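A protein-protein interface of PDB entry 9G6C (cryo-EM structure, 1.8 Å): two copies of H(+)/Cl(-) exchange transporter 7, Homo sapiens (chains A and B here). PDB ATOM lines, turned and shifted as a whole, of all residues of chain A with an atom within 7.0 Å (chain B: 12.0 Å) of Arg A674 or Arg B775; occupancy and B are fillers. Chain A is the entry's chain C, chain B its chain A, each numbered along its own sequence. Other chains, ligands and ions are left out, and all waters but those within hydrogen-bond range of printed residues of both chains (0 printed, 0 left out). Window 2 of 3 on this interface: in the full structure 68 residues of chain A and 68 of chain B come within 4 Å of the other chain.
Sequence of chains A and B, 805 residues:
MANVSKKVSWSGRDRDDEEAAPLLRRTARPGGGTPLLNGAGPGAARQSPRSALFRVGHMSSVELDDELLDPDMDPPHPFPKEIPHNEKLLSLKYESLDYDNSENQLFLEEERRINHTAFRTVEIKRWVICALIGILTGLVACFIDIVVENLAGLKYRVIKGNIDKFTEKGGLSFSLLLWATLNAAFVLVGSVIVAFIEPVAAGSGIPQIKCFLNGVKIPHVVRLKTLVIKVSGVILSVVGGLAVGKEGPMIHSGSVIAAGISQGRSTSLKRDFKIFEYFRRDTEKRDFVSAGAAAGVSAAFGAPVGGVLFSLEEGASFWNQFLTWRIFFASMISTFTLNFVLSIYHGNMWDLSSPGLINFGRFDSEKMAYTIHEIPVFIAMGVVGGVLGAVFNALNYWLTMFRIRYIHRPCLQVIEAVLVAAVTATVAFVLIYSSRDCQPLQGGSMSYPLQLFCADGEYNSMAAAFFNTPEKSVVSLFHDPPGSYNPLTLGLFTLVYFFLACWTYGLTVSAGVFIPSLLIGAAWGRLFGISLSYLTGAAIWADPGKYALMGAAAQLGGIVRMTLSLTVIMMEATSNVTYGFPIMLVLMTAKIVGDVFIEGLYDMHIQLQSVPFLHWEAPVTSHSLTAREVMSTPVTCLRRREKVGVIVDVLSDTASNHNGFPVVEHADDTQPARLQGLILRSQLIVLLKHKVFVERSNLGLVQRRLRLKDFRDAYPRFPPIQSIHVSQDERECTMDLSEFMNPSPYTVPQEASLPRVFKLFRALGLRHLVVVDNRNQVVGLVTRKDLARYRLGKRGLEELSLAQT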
ATOM      1  N   VAL A 663      18.154  26.041  24.668  1.00  0.00           N
ATOM      2  CA  VAL A 663      18.969  25.224  23.776  1.00  0.00           C
ATOM      3  C   VAL A 663      18.034  24.311  22.998  1.00  0.00           C
ATOM      4  O   VAL A 663      17.242  23.568  23.591  1.00  0.00           O
ATOM      5  CB  VAL A 663      20.018  24.416  24.554  1.00  0.00           C
ATOM      6  CG1 VAL A 663      20.845  23.577  23.597  1.00  0.00           C
ATOM      7  CG2 VAL A 663      20.906  25.344  25.365  1.00  0.00           C
ATOM      8  N   VAL A 664      18.120  24.360  21.668  1.00  0.00           N
ATOM      9  CA  VAL A 664      17.193  23.655  20.795  1.00  0.00           C
ATOM     10  C   VAL A 664      17.977  22.775  19.829  1.00  0.00           C
ATOM     11  O   VAL A 664      19.192  22.899  19.679  1.00  0.00           O
ATOM     12  CB  VAL A 664      16.274  24.620  20.021  1.00  0.00           C
ATOM     13  CG1 VAL A 664      15.395  25.403  20.983  1.00  0.00           C
ATOM     14  CG2 VAL A 664      17.101  25.561  19.161  1.00  0.00           C
ATOM     15  N   GLU A 665      17.252  21.874  19.172  1.00  0.00           N
ATOM     16  CA  GLU A 665      17.832  20.989  18.167  1.00  0.00           C
ATOM     17  C   GLU A 665      16.939  20.915  16.933  1.00  0.00           C
ATOM     18  O   GLU A 665      17.303  21.401  15.863  1.00  0.00           O
ATOM     19  CB  GLU A 665      18.049  19.589  18.741  1.00  0.00           C
ATOM     20  CG  GLU A 665      19.373  19.411  19.462  1.00  0.00           C
ATOM     21  CD  GLU A 665      20.040  18.091  19.135  1.00  0.00           C
ATOM     22  OE1 GLU A 665      20.670  17.991  18.063  1.00  0.00           O
ATOM     23  OE2 GLU A 665      19.934  17.153  19.953  1.00  0.00           O
ATOM     24  N   ALA A 673      13.192  23.805  16.382  1.00  0.00           N
ATOM     25  CA  ALA A 673      13.282  24.506  17.657  1.00  0.00           C
ATOM     26  C   ALA A 673      12.797  23.623  18.802  1.00  0.00           C
ATOM     27  O   ALA A 673      12.105  24.089  19.707  1.00  0.00           O
ATOM     28  CB  ALA A 673      12.484  25.799  17.609  1.00  0.00           C
ATOM     29  N   ARG A 674      13.165  22.346  18.756  1.00  0.00           N
ATOM     30  CA  ARG A 674      12.777  21.407  19.801  1.00  0.00           C
ATOM     31  C   ARG A 674      13.635  21.635  21.039  1.00  0.00           C
ATOM     32  O   ARG A 674      14.862  21.498  20.983  1.00  0.00           O
ATOM     33  CB  ARG A 674      12.919  19.974  19.299  1.00  0.00           C
ATOM     34  CG  ARG A 674      12.528  18.916  20.314  1.00  0.00           C
ATOM     35  CD  ARG A 674      12.410  17.554  19.656  1.00  0.00           C
ATOM     36  NE  ARG A 674      11.404  17.542  18.602  1.00  0.00           N
ATOM     37  CZ  ARG A 674      11.438  16.742  17.544  1.00  0.00           C
ATOM     38  NH1 ARG A 674      12.419  15.873  17.367  1.00  0.00           N
ATOM     39  NH2 ARG A 674      10.463  16.818  16.643  1.00  0.00           N
ATOM     40  N   LEU A 675      12.991  21.972  22.154  1.00  0.00           N
ATOM     41  CA  LEU A 675      13.715  22.353  23.360  1.00  0.00           C
ATOM     42  C   LEU A 675      14.570  21.205  23.882  1.00  0.00           C
ATOM     43  O   LEU A 675      14.111  20.065  23.983  1.00  0.00           O
ATOM     44  CB  LEU A 675      12.733  22.806  24.439  1.00  0.00           C
ATOM     45  CG  LEU A 675      13.365  23.289  25.746  1.00  0.00           C
ATOM     46  CD1 LEU A 675      14.261  24.492  25.501  1.00  0.00           C
ATOM     47  CD2 LEU A 675      12.291  23.613  26.767  1.00  0.00           C
ATOM     48  N   GLN A 676      15.819  21.519  24.218  1.00  0.00           N
ATOM     49  CA  GLN A 676      16.737  20.574  24.837  1.00  0.00           C
ATOM     50  C   GLN A 676      17.232  21.019  26.201  1.00  0.00           C
ATOM     51  O   GLN A 676      17.588  20.169  27.020  1.00  0.00           O
ATOM     52  CB  GLN A 676      17.956  20.336  23.934  1.00  0.00           C
ATOM     53  CG  GLN A 676      17.619  20.105  22.476  1.00  0.00           C
ATOM     54  CD  GLN A 676      16.927  18.781  22.238  1.00  0.00           C
ATOM     55  OE1 GLN A 676      17.467  17.721  22.552  1.00  0.00           O
ATOM     56  NE2 GLN A 676      15.729  18.835  21.670  1.00  0.00           N
ATOM     57  N   GLY A 677      17.269  22.319  26.465  1.00  0.00           N
ATOM     58  CA  GLY A 677      17.765  22.804  27.736  1.00  0.00           C
ATOM     59  C   GLY A 677      17.807  24.315  27.754  1.00  0.00           C
ATOM     60  O   GLY A 677      17.259  24.983  26.874  1.00  0.00           O
ATOM     61  N   ASN A 774       2.650  21.879  21.948  1.00  0.00           N
ATOM     62  CA  ASN A 774       2.438  20.464  22.225  1.00  0.00           C
ATOM     63  C   ASN A 774       3.502  19.564  21.609  1.00  0.00           C
ATOM     64  O   ASN A 774       3.530  18.370  21.920  1.00  0.00           O
ATOM     65  CB  ASN A 774       1.050  20.035  21.739  1.00  0.00           C
ATOM     66  CG  ASN A 774       0.975  19.899  20.233  1.00  0.00           C
ATOM     67  OD1 ASN A 774       0.371  18.962  19.711  1.00  0.00           O
ATOM     68  ND2 ASN A 774       1.593  20.836  19.524  1.00  0.00           N
ATOM     69  N   ARG A 775       4.377  20.100  20.756  1.00  0.00           N
ATOM     70  CA  ARG A 775       5.470  19.335  20.172  1.00  0.00           C
ATOM     71  C   ARG A 775       6.813  19.644  20.826  1.00  0.00           C
ATOM     72  O   ARG A 775       7.859  19.300  20.264  1.00  0.00           O
ATOM     73  CB  ARG A 775       5.553  19.585  18.666  1.00  0.00           C
ATOM     74  CG  ARG A 775       4.229  19.474  17.933  1.00  0.00           C
ATOM     75  CD  ARG A 775       4.444  19.025  16.489  1.00  0.00           C
ATOM     76  NE  ARG A 775       5.070  20.024  15.626  1.00  0.00           N
ATOM     77  CZ  ARG A 775       4.694  21.292  15.496  1.00  0.00           C
ATOM     78  NH1 ARG A 775       3.611  21.764  16.093  1.00  0.00           N
ATOM     79  NH2 ARG A 775       5.409  22.102  14.720  1.00  0.00           N
ATOM     80  N   ASN A 776       6.802  20.292  21.992  1.00  0.00           N
ATOM     81  CA  ASN A 776       8.022  20.688  22.700  1.00  0.00           C
ATOM     82  C   ASN A 776       8.878  21.627  21.850  1.00  0.00           C
ATOM     83  O   ASN A 776      10.109  21.585  21.889  1.00  0.00           O
ATOM     84  CB  ASN A 776       8.831  19.468  23.149  1.00  0.00           C
ATOM     85  CG  ASN A 776       9.727  19.766  24.335  1.00  0.00           C
ATOM     86  OD1 ASN A 776       9.372  20.552  25.214  1.00  0.00           O
ATOM     87  ND2 ASN A 776      10.897  19.140  24.364  1.00  0.00           N
ATOM     88  N   GLN A 777       8.219  22.480  21.072  1.00  0.00           N
ATOM     89  CA  GLN A 777       8.885  23.523  20.304  1.00  0.00           C
ATOM     90  C   GLN A 777       8.818  24.830  21.080  1.00  0.00           C
ATOM     91  O   GLN A 777       7.752  25.208  21.576  1.00  0.00           O
ATOM     92  CB  GLN A 777       8.242  23.691  18.927  1.00  0.00           C
ATOM     93  CG  GLN A 777       8.178  22.417  18.104  1.00  0.00           C
ATOM     94  CD  GLN A 777       9.532  22.004  17.562  1.00  0.00           C
ATOM     95  OE1 GLN A 777      10.260  22.819  16.995  1.00  0.00           O
ATOM     96  NE2 GLN A 777       9.877  20.734  17.736  1.00  0.00           N
ATOM     97  N   VAL A 778       9.956  25.514  21.187  1.00  0.00           N
ATOM     98  CA  VAL A 778      10.016  26.760  21.942  1.00  0.00           C
ATOM     99  C   VAL A 778       9.207  27.822  21.210  1.00  0.00           C
ATOM    100  O   VAL A 778       9.467  28.125  20.039  1.00  0.00           O
ATOM    101  CB  VAL A 778      11.468  27.210  22.146  1.00  0.00           C
ATOM    102  CG1 VAL A 778      11.510  28.549  22.864  1.00  0.00           C
ATOM    103  CG2 VAL A 778      12.242  26.158  22.919  1.00  0.00           C
ATOM    104  N   VAL B 663      -3.932  12.327  28.478  1.00  0.00           N
ATOM    105  CA  VAL B 663      -4.675  12.439  27.229  1.00  0.00           C
ATOM    106  C   VAL B 663      -3.685  12.735  26.112  1.00  0.00           C
ATOM    107  O   VAL B 663      -2.924  13.707  26.189  1.00  0.00           O
ATOM    108  CB  VAL B 663      -5.756  13.528  27.315  1.00  0.00           C
ATOM    109  CG1 VAL B 663      -6.493  13.637  25.995  1.00  0.00           C
ATOM    110  CG2 VAL B 663      -6.720  13.228  28.450  1.00  0.00           C
ATOM    111  N   VAL B 664      -3.693  11.901  25.072  1.00  0.00           N
ATOM    112  CA  VAL B 664      -2.707  11.971  24.005  1.00  0.00           C
ATOM    113  C   VAL B 664      -3.416  12.090  22.662  1.00  0.00           C
ATOM    114  O   VAL B 664      -4.628  11.903  22.550  1.00  0.00           O
ATOM    115  CB  VAL B 664      -1.760  10.753  24.007  1.00  0.00           C
ATOM    116  CG1 VAL B 664      -0.953  10.710  25.296  1.00  0.00           C
ATOM    117  CG2 VAL B 664      -2.550   9.469  23.823  1.00  0.00           C
ATOM    118  N   GLU B 665      -2.632  12.409  21.636  1.00  0.00           N
ATOM    119  CA  GLU B 665      -3.134  12.508  20.270  1.00  0.00           C
ATOM    120  C   GLU B 665      -2.172  11.845  19.291  1.00  0.00           C
ATOM    121  O   GLU B 665      -2.491  10.820  18.691  1.00  0.00           O
ATOM    122  CB  GLU B 665      -3.353  13.971  19.880  1.00  0.00           C
ATOM    123  CG  GLU B 665      -4.698  14.533  20.301  1.00  0.00           C
ATOM    124  CD  GLU B 665      -5.352  15.354  19.209  1.00  0.00           C
ATOM    125  OE1 GLU B 665      -5.892  14.755  18.254  1.00  0.00           O
ATOM    126  OE2 GLU B 665      -5.326  16.599  19.304  1.00  0.00           O
ATOM    127  N   ALA B 673       1.542   9.292  20.798  1.00  0.00           N
ATOM    128  CA  ALA B 673       1.377   9.486  22.234  1.00  0.00           C
ATOM    129  C   ALA B 673       1.807  10.888  22.650  1.00  0.00           C
ATOM    130  O   ALA B 673       2.439  11.071  23.690  1.00  0.00           O
ATOM    131  CB  ALA B 673       2.167   8.439  23.004  1.00  0.00           C
ATOM    132  N   ARG B 674       1.456  11.877  21.831  1.00  0.00           N
ATOM    133  CA  ARG B 674       1.795  13.263  22.128  1.00  0.00           C
ATOM    134  C   ARG B 674       0.869  13.799  23.213  1.00  0.00           C
ATOM    135  O   ARG B 674      -0.351  13.848  23.028  1.00  0.00           O
ATOM    136  CB  ARG B 674       1.691  14.111  20.865  1.00  0.00           C
ATOM    137  CG  ARG B 674       2.199  15.529  21.027  1.00  0.00           C
ATOM    138  CD  ARG B 674       2.304  16.225  19.682  1.00  0.00           C
ATOM    139  NE  ARG B 674       3.369  15.667  18.860  1.00  0.00           N
ATOM    140  CZ  ARG B 674       3.389  15.709  17.534  1.00  0.00           C
ATOM    141  NH1 ARG B 674       2.413  16.278  16.846  1.00  0.00           N
ATOM    142  NH2 ARG B 674       4.413  15.165  16.884  1.00  0.00           N
ATOM    143  N   LEU B 675       1.451  14.209  24.339  1.00  0.00           N
ATOM    144  CA  LEU B 675       0.657  14.619  25.490  1.00  0.00           C
ATOM    145  C   LEU B 675      -0.200  15.837  25.173  1.00  0.00           C
ATOM    146  O   LEU B 675       0.278  16.820  24.599  1.00  0.00           O
ATOM    147  CB  LEU B 675       1.572  14.920  26.676  1.00  0.00           C
ATOM    148  CG  LEU B 675       0.855  15.281  27.978  1.00  0.00           C
ATOM    149  CD1 LEU B 675      -0.055  14.149  28.428  1.00  0.00           C
ATOM    150  CD2 LEU B 675       1.859  15.628  29.060  1.00  0.00           C
ATOM    151  N   GLN B 676      -1.472  15.765  25.553  1.00  0.00           N
ATOM    152  CA  GLN B 676      -2.405  16.874  25.430  1.00  0.00           C
ATOM    153  C   GLN B 676      -2.993  17.314  26.759  1.00  0.00           C
ATOM    154  O   GLN B 676      -3.390  18.473  26.889  1.00  0.00           O
ATOM    155  CB  GLN B 676      -3.558  16.504  24.485  1.00  0.00           C
ATOM    156  CG  GLN B 676      -3.112  15.908  23.165  1.00  0.00           C
ATOM    157  CD  GLN B 676      -2.464  16.927  22.252  1.00  0.00           C
ATOM    158  OE1 GLN B 676      -3.091  17.909  21.856  1.00  0.00           O
ATOM    159  NE2 GLN B 676      -1.203  16.694  21.907  1.00  0.00           N
ATOM    160  N   GLY B 677      -3.063  16.422  27.739  1.00  0.00           N
ATOM    161  CA  GLY B 677      -3.632  16.764  29.025  1.00  0.00           C
ATOM    162  C   GLY B 677      -3.715  15.536  29.909  1.00  0.00           C
ATOM    163  O   GLY B 677      -3.132  14.491  29.610  1.00  0.00           O
ATOM    164  N   THR B 747       4.728  18.388  33.955  1.00  0.00           N
ATOM    165  CA  THR B 747       5.540  17.378  33.295  1.00  0.00           C
ATOM    166  C   THR B 747       7.007  17.574  33.647  1.00  0.00           C
ATOM    167  O   THR B 747       7.441  18.676  33.990  1.00  0.00           O
ATOM    168  CB  THR B 747       5.382  17.421  31.764  1.00  0.00           C
ATOM    169  OG1 THR B 747       6.072  18.561  31.240  1.00  0.00           O
ATOM    170  CG2 THR B 747       3.916  17.498  31.371  1.00  0.00           C
ATOM    171  N   VAL B 748       7.766  16.486  33.558  1.00  0.00           N
ATOM    172  CA  VAL B 748       9.212  16.523  33.747  1.00  0.00           C
ATOM    173  C   VAL B 748       9.866  15.746  32.611  1.00  0.00           C
ATOM    174  O   VAL B 748       9.266  14.796  32.087  1.00  0.00           O
ATOM    175  CB  VAL B 748       9.617  15.953  35.117  1.00  0.00           C
ATOM    176  CG1 VAL B 748       9.149  16.868  36.238  1.00  0.00           C
ATOM    177  CG2 VAL B 748       9.055  14.552  35.297  1.00  0.00           C
ATOM    178  N   PRO B 749      11.074  16.109  32.191  1.00  0.00           N
ATOM    179  CA  PRO B 749      11.771  15.315  31.175  1.00  0.00           C
ATOM    180  C   PRO B 749      12.218  13.974  31.737  1.00  0.00           C
ATOM    181  O   PRO B 749      12.268  13.756  32.949  1.00  0.00           O
ATOM    182  CB  PRO B 749      12.975  16.184  30.791  1.00  0.00           C
ATOM    183  CG  PRO B 749      12.680  17.544  31.326  1.00  0.00           C
ATOM    184  CD  PRO B 749      11.776  17.366  32.501  1.00  0.00           C
ATOM    185  N   GLN B 750      12.536  13.059  30.817  1.00  0.00           N
ATOM    186  CA  GLN B 750      12.993  11.731  31.215  1.00  0.00           C
ATOM    187  C   GLN B 750      14.257  11.804  32.062  1.00  0.00           C
ATOM    188  O   GLN B 750      14.446  10.996  32.979  1.00  0.00           O
ATOM    189  CB  GLN B 750      13.236  10.869  29.977  1.00  0.00           C
ATOM    190  CG  GLN B 750      12.482   9.555  29.977  1.00  0.00           C
ATOM    191  CD  GLN B 750      12.590   8.828  28.654  1.00  0.00           C
ATOM    192  OE1 GLN B 750      12.871   9.435  27.621  1.00  0.00           O
ATOM    193  NE2 GLN B 750      12.375   7.518  28.679  1.00  0.00           N
ATOM    194  N   GLU B 751      15.132  12.763  31.774  1.00  0.00           N
ATOM    195  CA  GLU B 751      16.418  12.878  32.447  1.00  0.00           C
ATOM    196  C   GLU B 751      16.377  13.776  33.676  1.00  0.00           C
ATOM    197  O   GLU B 751      17.426  14.007  34.287  1.00  0.00           O
ATOM    198  CB  GLU B 751      17.475  13.394  31.466  1.00  0.00           C
ATOM    199  CG  GLU B 751      17.308  14.857  31.092  1.00  0.00           C
ATOM    200  CD  GLU B 751      16.366  15.052  29.920  1.00  0.00           C
ATOM    201  OE1 GLU B 751      15.831  14.045  29.410  1.00  0.00           O
ATOM    202  OE2 GLU B 751      16.157  16.213  29.511  1.00  0.00           O
ATOM    203  N   VAL B 770       3.363  13.580  34.760  1.00  0.00           N
ATOM    204  CA  VAL B 770       3.624  12.921  33.486  1.00  0.00           C
ATOM    205  C   VAL B 770       5.085  13.115  33.110  1.00  0.00           C
ATOM    206  O   VAL B 770       5.597  14.239  33.113  1.00  0.00           O
ATOM    207  CB  VAL B 770       2.695  13.468  32.390  1.00  0.00           C
ATOM    208  CG1 VAL B 770       2.910  12.712  31.091  1.00  0.00           C
ATOM    209  CG2 VAL B 770       1.245  13.386  32.832  1.00  0.00           C
ATOM    210  N   VAL B 771       5.761  12.020  32.788  1.00  0.00           N
ATOM    211  CA  VAL B 771       7.127  12.072  32.283  1.00  0.00           C
ATOM    212  C   VAL B 771       7.079  12.016  30.764  1.00  0.00           C
ATOM    213  O   VAL B 771       6.445  11.125  30.186  1.00  0.00           O
ATOM    214  CB  VAL B 771       7.973  10.922  32.854  1.00  0.00           C
ATOM    215  CG1 VAL B 771       9.436  11.120  32.497  1.00  0.00           C
ATOM    216  CG2 VAL B 771       7.794  10.832  34.360  1.00  0.00           C
ATOM    217  N   VAL B 772       7.743  12.969  30.115  1.00  0.00           N
ATOM    218  CA  VAL B 772       7.723  13.075  28.665  1.00  0.00           C
ATOM    219  C   VAL B 772       9.150  13.001  28.141  1.00  0.00           C
ATOM    220  O   VAL B 772      10.120  13.275  28.853  1.00  0.00           O
ATOM    221  CB  VAL B 772       7.036  14.369  28.185  1.00  0.00           C
ATOM    222  CG1 VAL B 772       5.545  14.317  28.477  1.00  0.00           C
ATOM    223  CG2 VAL B 772       7.671  15.582  28.845  1.00  0.00           C
ATOM    224  N   ASP B 773       9.267  12.619  26.874  1.00  0.00           N
ATOM    225  CA  ASP B 773      10.550  12.585  26.192  1.00  0.00           C
ATOM    226  C   ASP B 773      10.797  13.931  25.507  1.00  0.00           C
ATOM    227  O   ASP B 773      10.099  14.917  25.758  1.00  0.00           O
ATOM    228  CB  ASP B 773      10.607  11.395  25.230  1.00  0.00           C
ATOM    229  CG  ASP B 773       9.664  11.538  24.041  1.00  0.00           C
ATOM    230  OD1 ASP B 773       8.958  12.561  23.925  1.00  0.00           O
ATOM    231  OD2 ASP B 773       9.633  10.608  23.209  1.00  0.00           O
ATOM    232  N   ASN B 774      11.802  13.983  24.632  1.00  0.00           N
ATOM    233  CA  ASN B 774      12.164  15.236  23.981  1.00  0.00           C
ATOM    234  C   ASN B 774      11.080  15.748  23.040  1.00  0.00           C
ATOM    235  O   ASN B 774      11.063  16.944  22.731  1.00  0.00           O
ATOM    236  CB  ASN B 774      13.481  15.063  23.221  1.00  0.00           C
ATOM    237  CG  ASN B 774      14.043  16.377  22.725  1.00  0.00           C
ATOM    238  OD1 ASN B 774      14.679  16.436  21.673  1.00  0.00           O
ATOM    239  ND2 ASN B 774      13.809  17.442  23.482  1.00  0.00           N
ATOM    240  N   ARG B 775      10.174  14.883  22.583  1.00  0.00           N
ATOM    241  CA  ARG B 775       9.136  15.265  21.634  1.00  0.00           C
ATOM    242  C   ARG B 775       7.757  15.367  22.279  1.00  0.00           C
ATOM    243  O   ARG B 775       6.745  15.266  21.580  1.00  0.00           O
ATOM    244  CB  ARG B 775       9.092  14.277  20.467  1.00  0.00           C
ATOM    245  CG  ARG B 775      10.446  13.966  19.858  1.00  0.00           C
ATOM    246  CD  ARG B 775      10.290  13.422  18.439  1.00  0.00           C
ATOM    247  NE  ARG B 775       9.719  12.078  18.366  1.00  0.00           N
ATOM    248  CZ  ARG B 775      10.120  11.019  19.061  1.00  0.00           C
ATOM    249  NH1 ARG B 775      11.183  11.060  19.850  1.00  0.00           N
ATOM    250  NH2 ARG B 775       9.451   9.876  18.940  1.00  0.00           N
ATOM    251  N   ASN B 776       7.702  15.558  23.599  1.00  0.00           N
ATOM    252  CA  ASN B 776       6.442  15.633  24.343  1.00  0.00           C
ATOM    253  C   ASN B 776       5.618  14.356  24.192  1.00  0.00           C
ATOM    254  O   ASN B 776       4.385  14.395  24.191  1.00  0.00           O
ATOM    255  CB  ASN B 776       5.618  16.858  23.930  1.00  0.00           C
ATOM    256  CG  ASN B 776       4.657  17.309  25.012  1.00  0.00           C
ATOM    257  OD1 ASN B 776       4.947  17.194  26.203  1.00  0.00           O
ATOM    258  ND2 ASN B 776       3.504  17.824  24.602  1.00  0.00           N
ATOM    259  N   GLN B 777       6.292  13.218  24.059  1.00  0.00           N
ATOM    260  CA  GLN B 777       5.630  11.922  24.028  1.00  0.00           C
ATOM    261  C   GLN B 777       5.622  11.333  25.432  1.00  0.00           C
ATOM    262  O   GLN B 777       6.649  11.336  26.117  1.00  0.00           O
ATOM    263  CB  GLN B 777       6.331  10.971  23.057  1.00  0.00           C
ATOM    264  CG  GLN B 777       6.439  11.491  21.633  1.00  0.00           C
ATOM    265  CD  GLN B 777       5.113  11.465  20.902  1.00  0.00           C
ATOM    266  OE1 GLN B 777       4.428  10.442  20.871  1.00  0.00           O
ATOM    267  NE2 GLN B 777       4.743  12.592  20.304  1.00  0.00           N
ATOM    268  N   VAL B 778       4.463  10.834  25.857  1.00  0.00           N
ATOM    269  CA  VAL B 778       4.333  10.280  27.200  1.00  0.00           C
ATOM    270  C   VAL B 778       5.162   9.007  27.291  1.00  0.00           C
ATOM    271  O   VAL B 778       4.963   8.060  26.521  1.00  0.00           O
ATOM    272  CB  VAL B 778       2.862  10.012  27.543  1.00  0.00           C
ATOM    273  CG1 VAL B 778       2.749   9.356  28.911  1.00  0.00           C
ATOM    274  CG2 VAL B 778       2.065  11.302  27.495  1.00  0.00           C
ATOM    275  N   VAL B 779       6.101   8.979  28.234  1.00  0.00           N
ATOM    276  CA  VAL B 779       6.953   7.816  28.448  1.00  0.00           C
ATOM    277  C   VAL B 779       6.802   7.219  29.837  1.00  0.00           C
ATOM    278  O   VAL B 779       7.228   6.073  30.048  1.00  0.00           O
ATOM    279  CB  VAL B 779       8.438   8.143  28.177  1.00  0.00           C
ATOM    280  CG1 VAL B 779       8.653   8.455  26.705  1.00  0.00           C
ATOM    281  CG2 VAL B 779       8.892   9.305  29.045  1.00  0.00           C
ATOM    282  N   GLY B 780       6.214   7.938  30.785  1.00  0.00           N
ATOM    283  CA  GLY B 780       6.041   7.406  32.125  1.00  0.00           C
ATOM    284  C   GLY B 780       5.116   8.284  32.934  1.00  0.00           C
ATOM    285  O   GLY B 780       4.768   9.399  32.534  1.00  0.00           O
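O of Asn A774 sits at hydrogen-bond distance from ND2 of Asn B776, 2.7 Å away. ND2 of Asn B774 lies within hydrogen-bond range of O of Leu A675 (2.7 Å). OD1 of Asn B774 sits at hydrogen-bond distance from NE2 of Gln A676, 2.6 Å away. The side-chain amide nitrogen (ND2) of Asn A776 sits at hydrogen-bond distance from the backbone carbonyl oxygen (O) of Asn B774 (2.7 Å).
N of Gln A676 is in hydrogen-bond range of O of Val A663 (2.6 Å). The side-chain carboxylate (OD1) of Asp B773 is in hydrogen-bond range of the backbone NH (N) of Asn B776. N of Arg A674 sits at hydrogen-bond distance from OE1 of Gln A777 (3.4 Å). N of Gln B676 sits at hydrogen-bond distance from O of Val B663, at 2.6 Å. O of Asn A776 lies within hydrogen-bond range of N of Leu A675, at 2.9 Å. N of Arg B674 sits at hydrogen-bond distance from OE1 of Gln B777.
Among the printed residues, merely in contact across the chains: Arg A674 with Asn B774 (3.2 Å), Arg A674 with Arg B775 (3.4 Å), Asn A774 with Arg B674 (3.3 Å), Asn A774 with Gln B676 (3.5 Å) and Arg A775 with Arg B674 (3.4 Å).
Of chain B, only Asn B774 and Arg B775 come within 4 Å of Arg A674. No residue of chain B comes within 4 Å of Val A664. No residue of chain B comes within 4 Å of Glu A665. Ala A673 touches none of the printed residues of chain B. Leu A675 touches one residue of chain B. Gly A677 touches none of the printed residues of chain B. Asn A774 touches just these residues of chain B: Arg B674 (3.3 Å), Gln B676 (3.5 Å) and Asn B776 (2.7 Å). Asn A776 touches just one residue of chain B: Asn B774. Printed residues of chain A within 4 Å of Arg B674: Asn A774 and Arg A775. Printed residues of chain B within 4 Å of Arg A775: Arg B674. Printed residues of chain A within 4 Å of Asn B776: Asn A774. Of the printed residues of chain A, Asn B774 touches Arg A674 (3.2 Å), Leu A675 (2.7 Å), Gln A676 (2.6 Å) and Asn A776 (2.7 Å). Of the printed residues of chain A, Gln B676 touches Asn A774 (3.5 Å). Val B778 touches none of the printed residues of chain A. The nearest residue of chain A that does not touch Arg B775 is Asn A776 (4.3 Å). The nearest printed residue of chain A that does not touch Gln B676 is Arg A775 (6.6 Å).
Of the 24 printed residues of chain B, 5 touch a printed residue of chain A. Printed residues of chain B that touch a printed residue of chain A: Arg B674, Gln B676, Asn B774, Arg B775 and Asn B776. Of the 13 printed residues of chain A, 6 touch a printed residue of chain B. Among the printed residues, 9 pairs touch across the chains.
Arg A674 touches Asn B774, and with the chains exchanged Asn A774 touches Arg B674. Arg A674 touches Arg B775, and with the chains exchanged Arg A775 touches Arg B674. Leu A675 touches Asn B774, but with the chains exchanged Asn A774 does not touch Leu B675 (4.4 Å). Asn A774 touches Asn B776, and with the chains exchanged Asn A776 touches Asn B774.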
